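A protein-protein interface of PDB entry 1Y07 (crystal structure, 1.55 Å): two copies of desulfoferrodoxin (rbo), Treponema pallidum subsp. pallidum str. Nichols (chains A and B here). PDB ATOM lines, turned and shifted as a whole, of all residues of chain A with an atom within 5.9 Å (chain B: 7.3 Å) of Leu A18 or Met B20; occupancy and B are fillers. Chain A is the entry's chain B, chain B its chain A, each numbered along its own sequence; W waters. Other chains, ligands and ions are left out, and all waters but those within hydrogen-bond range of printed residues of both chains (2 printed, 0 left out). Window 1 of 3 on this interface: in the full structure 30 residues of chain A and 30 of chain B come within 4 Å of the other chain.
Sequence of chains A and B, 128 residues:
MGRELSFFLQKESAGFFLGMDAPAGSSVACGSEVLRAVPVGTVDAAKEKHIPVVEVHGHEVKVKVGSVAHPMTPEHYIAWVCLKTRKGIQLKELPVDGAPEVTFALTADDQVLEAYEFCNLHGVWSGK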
ATOM      1  N   LEU A   5      30.790  -6.650  -8.756  1.00  0.00           N
ATOM      2  CA  LEU A   5      29.419  -6.179  -8.931  1.00  0.00           C
ATOM      3  C   LEU A   5      29.222  -4.760  -8.382  1.00  0.00           C
ATOM      4  O   LEU A   5      29.688  -4.436  -7.290  1.00  0.00           O
ATOM      5  CB  LEU A   5      28.454  -7.123  -8.227  1.00  0.00           C
ATOM      6  CG  LEU A   5      28.226  -8.444  -8.923  1.00  0.00           C
ATOM      7  CD1 LEU A   5      27.279  -9.250  -8.134  1.00  0.00           C
ATOM      8  CD2 LEU A   5      27.680  -8.240 -10.325  1.00  0.00           C
ATOM      9  N   SER A   6      28.560  -3.914  -9.168  1.00  0.00           N
ATOM     10  CA  SER A   6      28.108  -2.631  -8.714  1.00  0.00           C
ATOM     11  C   SER A   6      26.624  -2.508  -8.994  1.00  0.00           C
ATOM     12  O   SER A   6      26.094  -3.202  -9.874  1.00  0.00           O
ATOM     13  CB  SER A   6      28.843  -1.494  -9.443  1.00  0.00           C
ATOM     14  OG  SER A   6      29.004  -1.779 -10.840  1.00  0.00           O
ATOM     15  N   PHE A   7      25.984  -1.613  -8.235  1.00  0.00           N
ATOM     16  CA  PHE A   7      24.548  -1.413  -8.263  1.00  0.00           C
ATOM     17  C   PHE A   7      24.250   0.044  -8.362  1.00  0.00           C
ATOM     18  O   PHE A   7      24.835   0.845  -7.642  1.00  0.00           O
ATOM     19  CB  PHE A   7      23.930  -2.011  -6.996  1.00  0.00           C
ATOM     20  CG  PHE A   7      24.307  -3.455  -6.783  1.00  0.00           C
ATOM     21  CD1 PHE A   7      25.392  -3.811  -5.966  1.00  0.00           C
ATOM     22  CD2 PHE A   7      23.593  -4.464  -7.420  1.00  0.00           C
ATOM     23  CE1 PHE A   7      25.739  -5.176  -5.798  1.00  0.00           C
ATOM     24  CE2 PHE A   7      23.948  -5.804  -7.251  1.00  0.00           C
ATOM     25  CZ  PHE A   7      25.018  -6.141  -6.434  1.00  0.00           C
ATOM     26  N   PHE A   8      23.343   0.376  -9.256  1.00  0.00           N
ATOM     27  CA  PHE A   8      22.938   1.752  -9.536  1.00  0.00           C
ATOM     28  C   PHE A   8      21.402   1.751  -9.470  1.00  0.00           C
ATOM     29  O   PHE A   8      20.764   1.064 -10.260  1.00  0.00           O
ATOM     30  CB  PHE A   8      23.404   2.166 -10.929  1.00  0.00           C
ATOM     31  CG  PHE A   8      24.882   1.949 -11.154  1.00  0.00           C
ATOM     32  CD1 PHE A   8      25.377   0.700 -11.415  1.00  0.00           C
ATOM     33  CD2 PHE A   8      25.766   3.009 -11.089  1.00  0.00           C
ATOM     34  CE1 PHE A   8      26.735   0.497 -11.610  1.00  0.00           C
ATOM     35  CE2 PHE A   8      27.122   2.804 -11.269  1.00  0.00           C
ATOM     36  CZ  PHE A   8      27.599   1.524 -11.537  1.00  0.00           C
ATOM     37  N   ALA A  14      11.947   1.851  -8.546  1.00  0.00           N
ATOM     38  CA  ALA A  14      11.763   2.226  -9.952  1.00  0.00           C
ATOM     39  C   ALA A  14      12.721   1.494 -10.909  1.00  0.00           C
ATOM     40  O   ALA A  14      12.945   1.953 -12.030  1.00  0.00           O
ATOM     41  CB  ALA A  14      11.893   3.751 -10.125  1.00  0.00           C
ATOM     42  N   GLY A  15      13.296   0.365 -10.498  1.00  0.00           N
ATOM     43  CA  GLY A  15      14.274  -0.302 -11.337  1.00  0.00           C
ATOM     44  C   GLY A  15      15.704   0.137 -11.030  1.00  0.00           C
ATOM     45  O   GLY A  15      15.982   0.980 -10.154  1.00  0.00           O
ATOM     46  N   PHE A  16      16.646  -0.456 -11.753  1.00  0.00           N
ATOM     47  CA  PHE A  16      18.028  -0.306 -11.403  1.00  0.00           C
ATOM     48  C   PHE A  16      18.917  -0.947 -12.445  1.00  0.00           C
ATOM     49  O   PHE A  16      18.455  -1.573 -13.405  1.00  0.00           O
ATOM     50  CB  PHE A  16      18.311  -0.959 -10.028  1.00  0.00           C
ATOM     51  CG  PHE A  16      17.776  -2.347  -9.904  1.00  0.00           C
ATOM     52  CD1 PHE A  16      18.604  -3.419  -9.898  1.00  0.00           C
ATOM     53  CD2 PHE A  16      16.398  -2.570  -9.753  1.00  0.00           C
ATOM     54  CE1 PHE A  16      18.089  -4.694  -9.750  1.00  0.00           C
ATOM     55  CE2 PHE A  16      15.896  -3.855  -9.632  1.00  0.00           C
ATOM     56  CZ  PHE A  16      16.746  -4.905  -9.635  1.00  0.00           C
ATOM     57  N   PHE A  17      20.209  -0.777 -12.232  1.00  0.00           N
ATOM     58  CA  PHE A  17      21.223  -1.365 -13.072  1.00  0.00           C
ATOM     59  C   PHE A  17      22.222  -2.130 -12.263  1.00  0.00           C
ATOM     60  O   PHE A  17      22.580  -1.739 -11.161  1.00  0.00           O
ATOM     61  CB  PHE A  17      21.957  -0.291 -13.879  1.00  0.00           C
ATOM     62  CG  PHE A  17      21.016   0.624 -14.639  1.00  0.00           C
ATOM     63  CD1 PHE A  17      20.270   1.602 -13.949  1.00  0.00           C
ATOM     64  CD2 PHE A  17      20.885   0.515 -16.019  1.00  0.00           C
ATOM     65  CE1 PHE A  17      19.435   2.444 -14.640  1.00  0.00           C
ATOM     66  CE2 PHE A  17      20.035   1.370 -16.717  1.00  0.00           C
ATOM     67  CZ  PHE A  17      19.295   2.289 -16.025  1.00  0.00           C
ATOM     68  N   LEU A  18      22.659  -3.233 -12.839  1.00  0.00           N
ATOM     69  CA  LEU A  18      23.727  -4.076 -12.282  1.00  0.00           C
ATOM     70  C   LEU A  18      24.928  -3.941 -13.207  1.00  0.00           C
ATOM     71  O   LEU A  18      24.818  -4.181 -14.393  1.00  0.00           O
ATOM     72  CB  LEU A  18      23.212  -5.549 -12.222  1.00  0.00           C
ATOM     73  CG  LEU A  18      24.029  -6.755 -11.756  1.00  0.00           C
ATOM     74  CD1 LEU A  18      23.022  -7.758 -11.258  1.00  0.00           C
ATOM     75  CD2 LEU A  18      24.869  -7.417 -12.857  1.00  0.00           C
ATOM     76  N   GLY A  19      26.059  -3.498 -12.678  1.00  0.00           N
ATOM     77  CA  GLY A  19      27.298  -3.438 -13.421  1.00  0.00           C
ATOM     78  C   GLY A  19      28.269  -4.556 -13.075  1.00  0.00           C
ATOM     79  O   GLY A  19      28.411  -4.955 -11.921  1.00  0.00           O
ATOM     80  N   MET A  20      28.872  -5.129 -14.107  1.00  0.00           N
ATOM     81  CA  MET A  20      29.908  -6.141 -13.921  1.00  0.00           C
ATOM     82  C   MET A  20      31.244  -5.542 -14.394  1.00  0.00           C
ATOM     83  O   MET A  20      31.389  -5.168 -15.572  1.00  0.00           O
ATOM     84  CB  MET A  20      29.565  -7.451 -14.636  1.00  0.00           C
ATOM     85  CG  MET A  20      30.679  -8.531 -14.454  1.00  0.00           C
ATOM     86  SD  MET A  20      31.049  -9.119 -12.718  1.00  0.00           S
ATOM     87  CE  MET A  20      29.629 -10.221 -12.369  1.00  0.00           C
ATOM     88  N   CYS A  82      20.923 -10.524  -4.635  1.00  0.00           N
ATOM     89  CA  CYS A  82      21.761 -10.878  -5.789  1.00  0.00           C
ATOM     90  C   CYS A  82      22.823 -11.878  -5.306  1.00  0.00           C
ATOM     91  O   CYS A  82      23.398 -11.705  -4.238  1.00  0.00           O
ATOM     92  CB  CYS A  82      22.395  -9.617  -6.359  1.00  0.00           C
ATOM     93  SG  CYS A  82      23.602  -9.875  -7.656  1.00  0.00           S
ATOM     94  N   ILE A  89      25.797 -14.939 -12.232  1.00  0.00           N
ATOM     95  CA  ILE A  89      25.104 -14.061 -11.279  1.00  0.00           C
ATOM     96  C   ILE A  89      23.617 -14.404 -11.354  1.00  0.00           C
ATOM     97  O   ILE A  89      23.132 -14.874 -12.403  1.00  0.00           O
ATOM     98  CB  ILE A  89      25.324 -12.520 -11.517  1.00  0.00           C
ATOM     99  CG1 ILE A  89      24.793 -12.053 -12.865  1.00  0.00           C
ATOM    100  CG2 ILE A  89      26.774 -12.136 -11.247  1.00  0.00           C
ATOM    101  CD1 ILE A  89      24.810 -10.595 -13.029  1.00  0.00           C
ATOM    102  N   GLN A  90      22.919 -14.148 -10.258  1.00  0.00           N
ATOM    103  CA  GLN A  90      21.469 -14.240 -10.191  1.00  0.00           C
ATOM    104  C   GLN A  90      20.913 -13.093  -9.378  1.00  0.00           C
ATOM    105  O   GLN A  90      21.580 -12.559  -8.508  1.00  0.00           O
ATOM    106  CB  GLN A  90      21.026 -15.508  -9.486  1.00  0.00           C
ATOM    107  CG  GLN A  90      21.640 -16.719 -10.104  1.00  0.00           C
ATOM    108  CD  GLN A  90      20.868 -18.038  -9.723  1.00  0.00           C
ATOM    109  OE1 GLN A  90      19.684 -18.039  -9.701  1.00  0.00           O
ATOM    110  NE2 GLN A  90      21.613 -19.110  -9.437  1.00  0.00           N
ATOM    111  N   LEU A  91      19.684 -12.717  -9.675  1.00  0.00           N
ATOM    112  CA  LEU A  91      19.012 -11.747  -8.861  1.00  0.00           C
ATOM    113  C   LEU A  91      17.550 -12.104  -8.797  1.00  0.00           C
ATOM    114  O   LEU A  91      16.935 -12.459  -9.798  1.00  0.00           O
ATOM    115  CB  LEU A  91      19.281 -10.332  -9.352  1.00  0.00           C
ATOM    116  CG  LEU A  91      18.771  -9.145  -8.498  1.00  0.00           C
ATOM    117  CD1 LEU A  91      19.605  -7.892  -8.723  1.00  0.00           C
ATOM    118  CD2 LEU A  91      17.347  -8.951  -8.832  1.00  0.00           C
ATOM    119  N   GLU A  93      13.937 -10.620  -6.900  1.00  0.00           N
ATOM    120  CA  GLU A  93      13.209  -9.691  -6.045  1.00  0.00           C
ATOM    121  C   GLU A  93      12.446 -10.495  -4.993  1.00  0.00           C
ATOM    122  O   GLU A  93      12.021 -11.614  -5.239  1.00  0.00           O
ATOM    123  CB  GLU A  93      12.273  -8.829  -6.874  1.00  0.00           C
ATOM    124  CG  GLU A  93      13.052  -7.959  -7.829  1.00  0.00           C
ATOM    125  CD  GLU A  93      12.225  -7.092  -8.783  1.00  0.00           C
ATOM    126  OE1 GLU A  93      11.030  -7.391  -8.974  1.00  0.00           O
ATOM    127  OE2 GLU A  93      12.793  -6.126  -9.370  1.00  0.00           O
ATOM    128  N   ARG B   3      10.523  -7.580 -14.805  1.00  0.00           N
ATOM    129  CA  ARG B   3      11.064  -6.298 -15.368  1.00  0.00           C
ATOM    130  C   ARG B   3      11.426  -6.458 -16.857  1.00  0.00           C
ATOM    131  O   ARG B   3      11.747  -7.544 -17.327  1.00  0.00           O
ATOM    132  CB  ARG B   3      12.353  -5.856 -14.627  1.00  0.00           C
ATOM    133  CG  ARG B   3      12.279  -5.728 -13.099  1.00  0.00           C
ATOM    134  CD  ARG B   3      11.554  -4.475 -12.636  1.00  0.00           C
ATOM    135  NE  ARG B   3      11.743  -4.207 -11.217  1.00  0.00           N
ATOM    136  CZ  ARG B   3      11.627  -3.006 -10.650  1.00  0.00           C
ATOM    137  NH1 ARG B   3      11.294  -1.936 -11.372  1.00  0.00           N
ATOM    138  NH2 ARG B   3      11.813  -2.870  -9.326  1.00  0.00           N
ATOM    139  N   GLU B   4      11.444  -5.358 -17.593  1.00  0.00           N
ATOM    140  CA  GLU B   4      12.099  -5.365 -18.891  1.00  0.00           C
ATOM    141  C   GLU B   4      13.623  -5.235 -18.709  1.00  0.00           C
ATOM    142  O   GLU B   4      14.121  -4.356 -18.013  1.00  0.00           O
ATOM    143  CB  GLU B   4      11.593  -4.252 -19.784  1.00  0.00           C
ATOM    144  CG  GLU B   4      10.105  -4.400 -20.125  1.00  0.00           C
ATOM    145  CD  GLU B   4       9.761  -5.584 -21.034  1.00  0.00           C
ATOM    146  OE1 GLU B   4      10.648  -6.147 -21.761  1.00  0.00           O
ATOM    147  OE2 GLU B   4       8.550  -5.936 -21.031  1.00  0.00           O
ATOM    148  N   LEU B   5      14.328  -6.110 -19.394  1.00  0.00           N
ATOM    149  CA  LEU B   5      15.773  -6.208 -19.374  1.00  0.00           C
ATOM    150  C   LEU B   5      16.380  -5.469 -20.535  1.00  0.00           C
ATOM    151  O   LEU B   5      15.873  -5.483 -21.675  1.00  0.00           O
ATOM    152  CB  LEU B   5      16.252  -7.678 -19.409  1.00  0.00           C
ATOM    153  CG  LEU B   5      15.687  -8.535 -18.313  1.00  0.00           C
ATOM    154  CD1 LEU B   5      16.249  -9.951 -18.486  1.00  0.00           C
ATOM    155  CD2 LEU B   5      16.065  -7.972 -16.923  1.00  0.00           C
ATOM    156  N   SER B   6      17.485  -4.818 -20.243  1.00  0.00           N
ATOM    157  CA  SER B   6      18.262  -4.102 -21.265  1.00  0.00           C
ATOM    158  C   SER B   6      19.720  -4.393 -20.972  1.00  0.00           C
ATOM    159  O   SER B   6      20.093  -4.745 -19.852  1.00  0.00           O
ATOM    160  CB  SER B   6      18.021  -2.595 -21.213  1.00  0.00           C
ATOM    161  OG  SER B   6      18.126  -2.122 -19.915  1.00  0.00           O
ATOM    162  N   PHE B   8      23.725  -3.051 -21.609  1.00  0.00           N
ATOM    163  CA  PHE B   8      24.674  -1.976 -21.949  1.00  0.00           C
ATOM    164  C   PHE B   8      26.084  -2.609 -21.982  1.00  0.00           C
ATOM    165  O   PHE B   8      26.562  -3.132 -20.983  1.00  0.00           O
ATOM    166  CB  PHE B   8      24.585  -0.902 -20.906  1.00  0.00           C
ATOM    167  CG  PHE B   8      23.179  -0.367 -20.734  1.00  0.00           C
ATOM    168  CD1 PHE B   8      22.232  -1.034 -19.949  1.00  0.00           C
ATOM    169  CD2 PHE B   8      22.819   0.855 -21.354  1.00  0.00           C
ATOM    170  CE1 PHE B   8      20.914  -0.523 -19.829  1.00  0.00           C
ATOM    171  CE2 PHE B   8      21.514   1.377 -21.222  1.00  0.00           C
ATOM    172  CZ  PHE B   8      20.569   0.698 -20.457  1.00  0.00           C
ATOM    173  N   PHE B  16      29.757  -5.964 -18.200  1.00  0.00           N
ATOM    174  CA  PHE B  16      28.472  -5.628 -18.855  1.00  0.00           C
ATOM    175  C   PHE B  16      27.750  -4.730 -17.833  1.00  0.00           C
ATOM    176  O   PHE B  16      28.122  -4.724 -16.662  1.00  0.00           O
ATOM    177  CB  PHE B  16      27.625  -6.915 -19.206  1.00  0.00           C
ATOM    178  CG  PHE B  16      27.511  -7.905 -18.047  1.00  0.00           C
ATOM    179  CD1 PHE B  16      26.576  -7.702 -17.017  1.00  0.00           C
ATOM    180  CD2 PHE B  16      28.365  -9.029 -17.971  1.00  0.00           C
ATOM    181  CE1 PHE B  16      26.533  -8.578 -15.899  1.00  0.00           C
ATOM    182  CE2 PHE B  16      28.292  -9.928 -16.869  1.00  0.00           C
ATOM    183  CZ  PHE B  16      27.337  -9.678 -15.835  1.00  0.00           C
ATOM    184  N   PHE B  17      26.712  -4.015 -18.265  1.00  0.00           N
ATOM    185  CA  PHE B  17      25.665  -3.582 -17.336  1.00  0.00           C
ATOM    186  C   PHE B  17      24.341  -4.194 -17.779  1.00  0.00           C
ATOM    187  O   PHE B  17      24.022  -4.169 -18.919  1.00  0.00           O
ATOM    188  CB  PHE B  17      25.491  -2.074 -17.242  1.00  0.00           C
ATOM    189  CG  PHE B  17      26.726  -1.350 -16.862  1.00  0.00           C
ATOM    190  CD1 PHE B  17      27.767  -1.271 -17.769  1.00  0.00           C
ATOM    191  CD2 PHE B  17      26.855  -0.773 -15.615  1.00  0.00           C
ATOM    192  CE1 PHE B  17      28.939  -0.605 -17.458  1.00  0.00           C
ATOM    193  CE2 PHE B  17      28.052  -0.084 -15.275  1.00  0.00           C
ATOM    194  CZ  PHE B  17      29.087  -0.028 -16.206  1.00  0.00           C
ATOM    195  N   LEU B  18      23.526  -4.564 -16.814  1.00  0.00           N
ATOM    196  CA  LEU B  18      22.199  -5.081 -17.025  1.00  0.00           C
ATOM    197  C   LEU B  18      21.226  -4.063 -16.481  1.00  0.00           C
ATOM    198  O   LEU B  18      21.341  -3.632 -15.328  1.00  0.00           O
ATOM    199  CB  LEU B  18      22.085  -6.384 -16.229  1.00  0.00           C
ATOM    200  CG  LEU B  18      21.286  -7.473 -16.866  1.00  0.00           C
ATOM    201  CD1 LEU B  18      21.722  -8.782 -16.134  1.00  0.00           C
ATOM    202  CD2 LEU B  18      19.849  -7.205 -16.722  1.00  0.00           C
ATOM    203  N   GLY B  19      20.241  -3.668 -17.283  1.00  0.00           N
ATOM    204  CA  GLY B  19      19.195  -2.804 -16.810  1.00  0.00           C
ATOM    205  C   GLY B  19      17.893  -3.499 -16.598  1.00  0.00           C
ATOM    206  O   GLY B  19      17.564  -4.411 -17.313  1.00  0.00           O
ATOM    207  N   MET B  20      17.214  -3.110 -15.530  1.00  0.00           N
ATOM    208  CA  MET B  20      15.913  -3.647 -15.133  1.00  0.00           C
ATOM    209  C   MET B  20      14.999  -2.433 -15.067  1.00  0.00           C
ATOM    210  O   MET B  20      15.171  -1.580 -14.237  1.00  0.00           O
ATOM    211  CB  MET B  20      16.027  -4.379 -13.799  1.00  0.00           C
ATOM    212  CG  MET B  20      16.651  -5.766 -13.970  1.00  0.00           C
ATOM    213  SD  MET B  20      17.737  -6.341 -12.615  1.00  0.00           S
ATOM    214  CE  MET B  20      19.087  -4.961 -12.666  1.00  0.00           C
ATOM    215  N   ASP B  21      14.031  -2.384 -15.982  1.00  0.00           N
ATOM    216  CA  ASP B  21      13.143  -1.231 -16.164  1.00  0.00           C
ATOM    217  C   ASP B  21      13.895   0.057 -16.370  1.00  0.00           C
ATOM    218  O   ASP B  21      13.544   1.101 -15.834  1.00  0.00           O
ATOM    219  CB  ASP B  21      12.181  -1.087 -14.959  1.00  0.00           C
ATOM    220  CG  ASP B  21      11.098  -2.056 -14.988  1.00  0.00           C
ATOM    221  OD1 ASP B  21      11.049  -2.922 -15.906  1.00  0.00           O
ATOM    222  OD2 ASP B  21      10.204  -2.016 -14.099  1.00  0.00           O
ATOM    223  N   ALA B  22      14.937   0.004 -17.181  1.00  0.00           N
ATOM    224  CA  ALA B  22      15.656   1.208 -17.513  1.00  0.00           C
ATOM    225  C   ALA B  22      14.858   2.075 -18.480  1.00  0.00           C
ATOM    226  O   ALA B  22      14.319   1.549 -19.467  1.00  0.00           O
ATOM    227  CB  ALA B  22      16.997   0.862 -18.124  1.00  0.00           C
ATOM    228  N   PRO B  23      14.796   3.382 -18.206  1.00  0.00           N
ATOM    229  CA  PRO B  23      14.128   4.302 -19.118  1.00  0.00           C
ATOM    230  C   PRO B  23      14.803   4.252 -20.469  1.00  0.00           C
ATOM    231  O   PRO B  23      16.046   4.125 -20.535  1.00  0.00           O
ATOM    232  CB  PRO B  23      14.331   5.696 -18.475  1.00  0.00           C
ATOM    233  CG  PRO B  23      14.630   5.471 -17.027  1.00  0.00           C
ATOM    234  CD  PRO B  23      15.303   4.080 -17.011  1.00  0.00           C
ATOM    235  N   ILE B  89      16.368 -13.333 -12.495  1.00  0.00           N
ATOM    236  CA  ILE B  89      17.241 -13.252 -13.632  1.00  0.00           C
ATOM    237  C   ILE B  89      18.553 -14.009 -13.323  1.00  0.00           C
ATOM    238  O   ILE B  89      18.967 -14.134 -12.160  1.00  0.00           O
ATOM    239  CB  ILE B  89      17.505 -11.798 -14.121  1.00  0.00           C
ATOM    240  CG1 ILE B  89      18.231 -10.958 -13.082  1.00  0.00           C
ATOM    241  CG2 ILE B  89      16.204 -11.168 -14.560  1.00  0.00           C
ATOM    242  CD1 ILE B  89      18.796  -9.699 -13.712  1.00  0.00           C
ATOM    243  N   LEU B  91      22.623 -14.683 -15.323  1.00  0.00           N
ATOM    244  CA  LEU B  91      23.562 -14.455 -16.408  1.00  0.00           C
ATOM    245  C   LEU B  91      24.832 -15.277 -16.180  1.00  0.00           C
ATOM    246  O   LEU B  91      25.387 -15.245 -15.115  1.00  0.00           O
ATOM    247  CB  LEU B  91      23.874 -12.993 -16.520  1.00  0.00           C
ATOM    248  CG  LEU B  91      24.578 -12.617 -17.830  1.00  0.00           C
ATOM    249  CD1 LEU B  91      24.244 -11.218 -18.239  1.00  0.00           C
ATOM    250  CD2 LEU B  91      26.092 -12.774 -17.764  1.00  0.00           C
HETATM  251  O   HOH W   1      17.622 -16.187 -10.317  1.00  0.00           O
HETATM  252  O   HOH W   2      12.096   3.419 -14.803  1.00  0.00           O
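The backbone NH (N) of Ile B89 lies within hydrogen-bond range of the backbone carbonyl oxygen (O) of Leu A91 (2.9 Å).
The backbone NH (N) of Gly A15 sits close to the guanidinium group (NH1) of Arg B3.
The backbone NH (N) of Ile A89 is in hydrogen-bond range of the backbone carbonyl oxygen (O) of Leu B91 (2.9 Å).
The backbone carbonyl oxygen of Leu A18 is in hydrogen-bond range of the backbone NH of Leu B18 (2.8 Å).
The backbone carbonyl oxygen (O) of Phe A16 sits at hydrogen-bond distance from the backbone NH (N) of Met B20 (2.9 Å).
OE2 of Glu A93 is in salt-bridge range of NE of Arg B3 (2.9 Å).
The backbone NH of Met A20 is in hydrogen-bond range of the backbone carbonyl oxygen of Phe B16.
The backbone carbonyl oxygen of Phe A8 lies within hydrogen-bond range of the backbone NH of Phe A17 (2.8 Å).
The backbone carbonyl oxygen of Glu B4 lies within hydrogen-bond range of the backbone NH of Asp B21.
The guanidinium group (NH1) of Arg B3 lies within salt-bridge range of the side-chain carboxylate (OD2) of Asp B21 (2.9 Å).
The backbone NH of Gly B19 sits at hydrogen-bond distance from the backbone carbonyl oxygen of Ser B6 (2.8 Å).
The side-chain sulfur (SG) of Cys A82 lies close to the backbone carbonyl oxygen (O) of Gln A90.
O of Ser A6 lies within hydrogen-bond range of N of Gly A19 (2.8 Å).
Among the printed residues, pairs that only touch across the chains: Phe A8 with Phe B17 (3.9 Å), Ala A14 with Arg B3 (3.7 Å), Ala A14 with Asp B21 (3.9 Å), Gly A15 with Met B20 (3.3 Å), Phe A16 with Gly B19 (3.7 Å), Phe A17 with Phe B8 (3.7 Å), Phe A17 with Leu B18 (3.2 Å), Phe A17 with Gly B19 (3.8 Å), Phe A17 with Ala B22 (3.4 Å), Leu A18 with Phe B16 (3.7 Å), Leu A18 with Phe B17 (3.1 Å), Leu A18 with Met B20 (3.97 Å), Gly A19 with Phe B16 (3.6 Å), Gly A19 with Phe B17 (3.5 Å), Ile A89 with Phe B16 (3.9 Å) and Gln A90 with Ile B89 (3.2 Å).
Leu A5 touches none of the printed residues of chain B.
Printed residues of chain B within 4 Å of Phe A17: Phe B8 (3.7 Å), Leu B18 (3.2 Å), Gly B19 (3.8 Å) and Ala B22 (3.4 Å).
Leu A18 touches four residues of chain B.
Of the printed residues of chain A, Leu B18 touches Phe A17 and Leu A18.
Of chain A, only Gly A15, Phe A16 and Leu A18 come within 4 Å of Met B20.
Pro B23 touches none of the printed residues of chain A.
Printed residues of chain A within 4 Å of Leu B91: Ile A89.
The nearest residue of chain A that does not touch Met B20 is Phe A17 (4.2 Å).
Hydrophobic or aromatic side chains of chain A within 4 Å of the printed part of chain B: Phe A8, Phe A16, Phe A17, Leu A18, Met A20, Ile A89 and Leu A91.
Of the 15 printed residues of chain B, 11 touch a printed residue of chain A.
Among the printed residues, Asp or Glu carboxylates within 4 Å of a Lys or Arg side-chain nitrogen of the other chain: Glu A93 with Arg B3.
Phe A16 touches Gly B19, and with the chains exchanged Gly A19 touches Phe B16.
Phe A17 touches Leu B18, and with the chains exchanged Leu A18 touches Phe B17.
Leu B18 touches its own counterpart, Leu A18.
Ile A89 touches Leu B91, and with the chains exchanged Leu A91 touches Ile B89.
Water W1 bridges the side-chain amide oxygen of Gln A90 and the backbone carbonyl oxygen of Ile B89.
Water W2 bridges the backbone carbonyl oxygen of Asp B21 (2.9 Å) and the backbone carbonyl oxygen of Ala A14 (3.2 Å).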
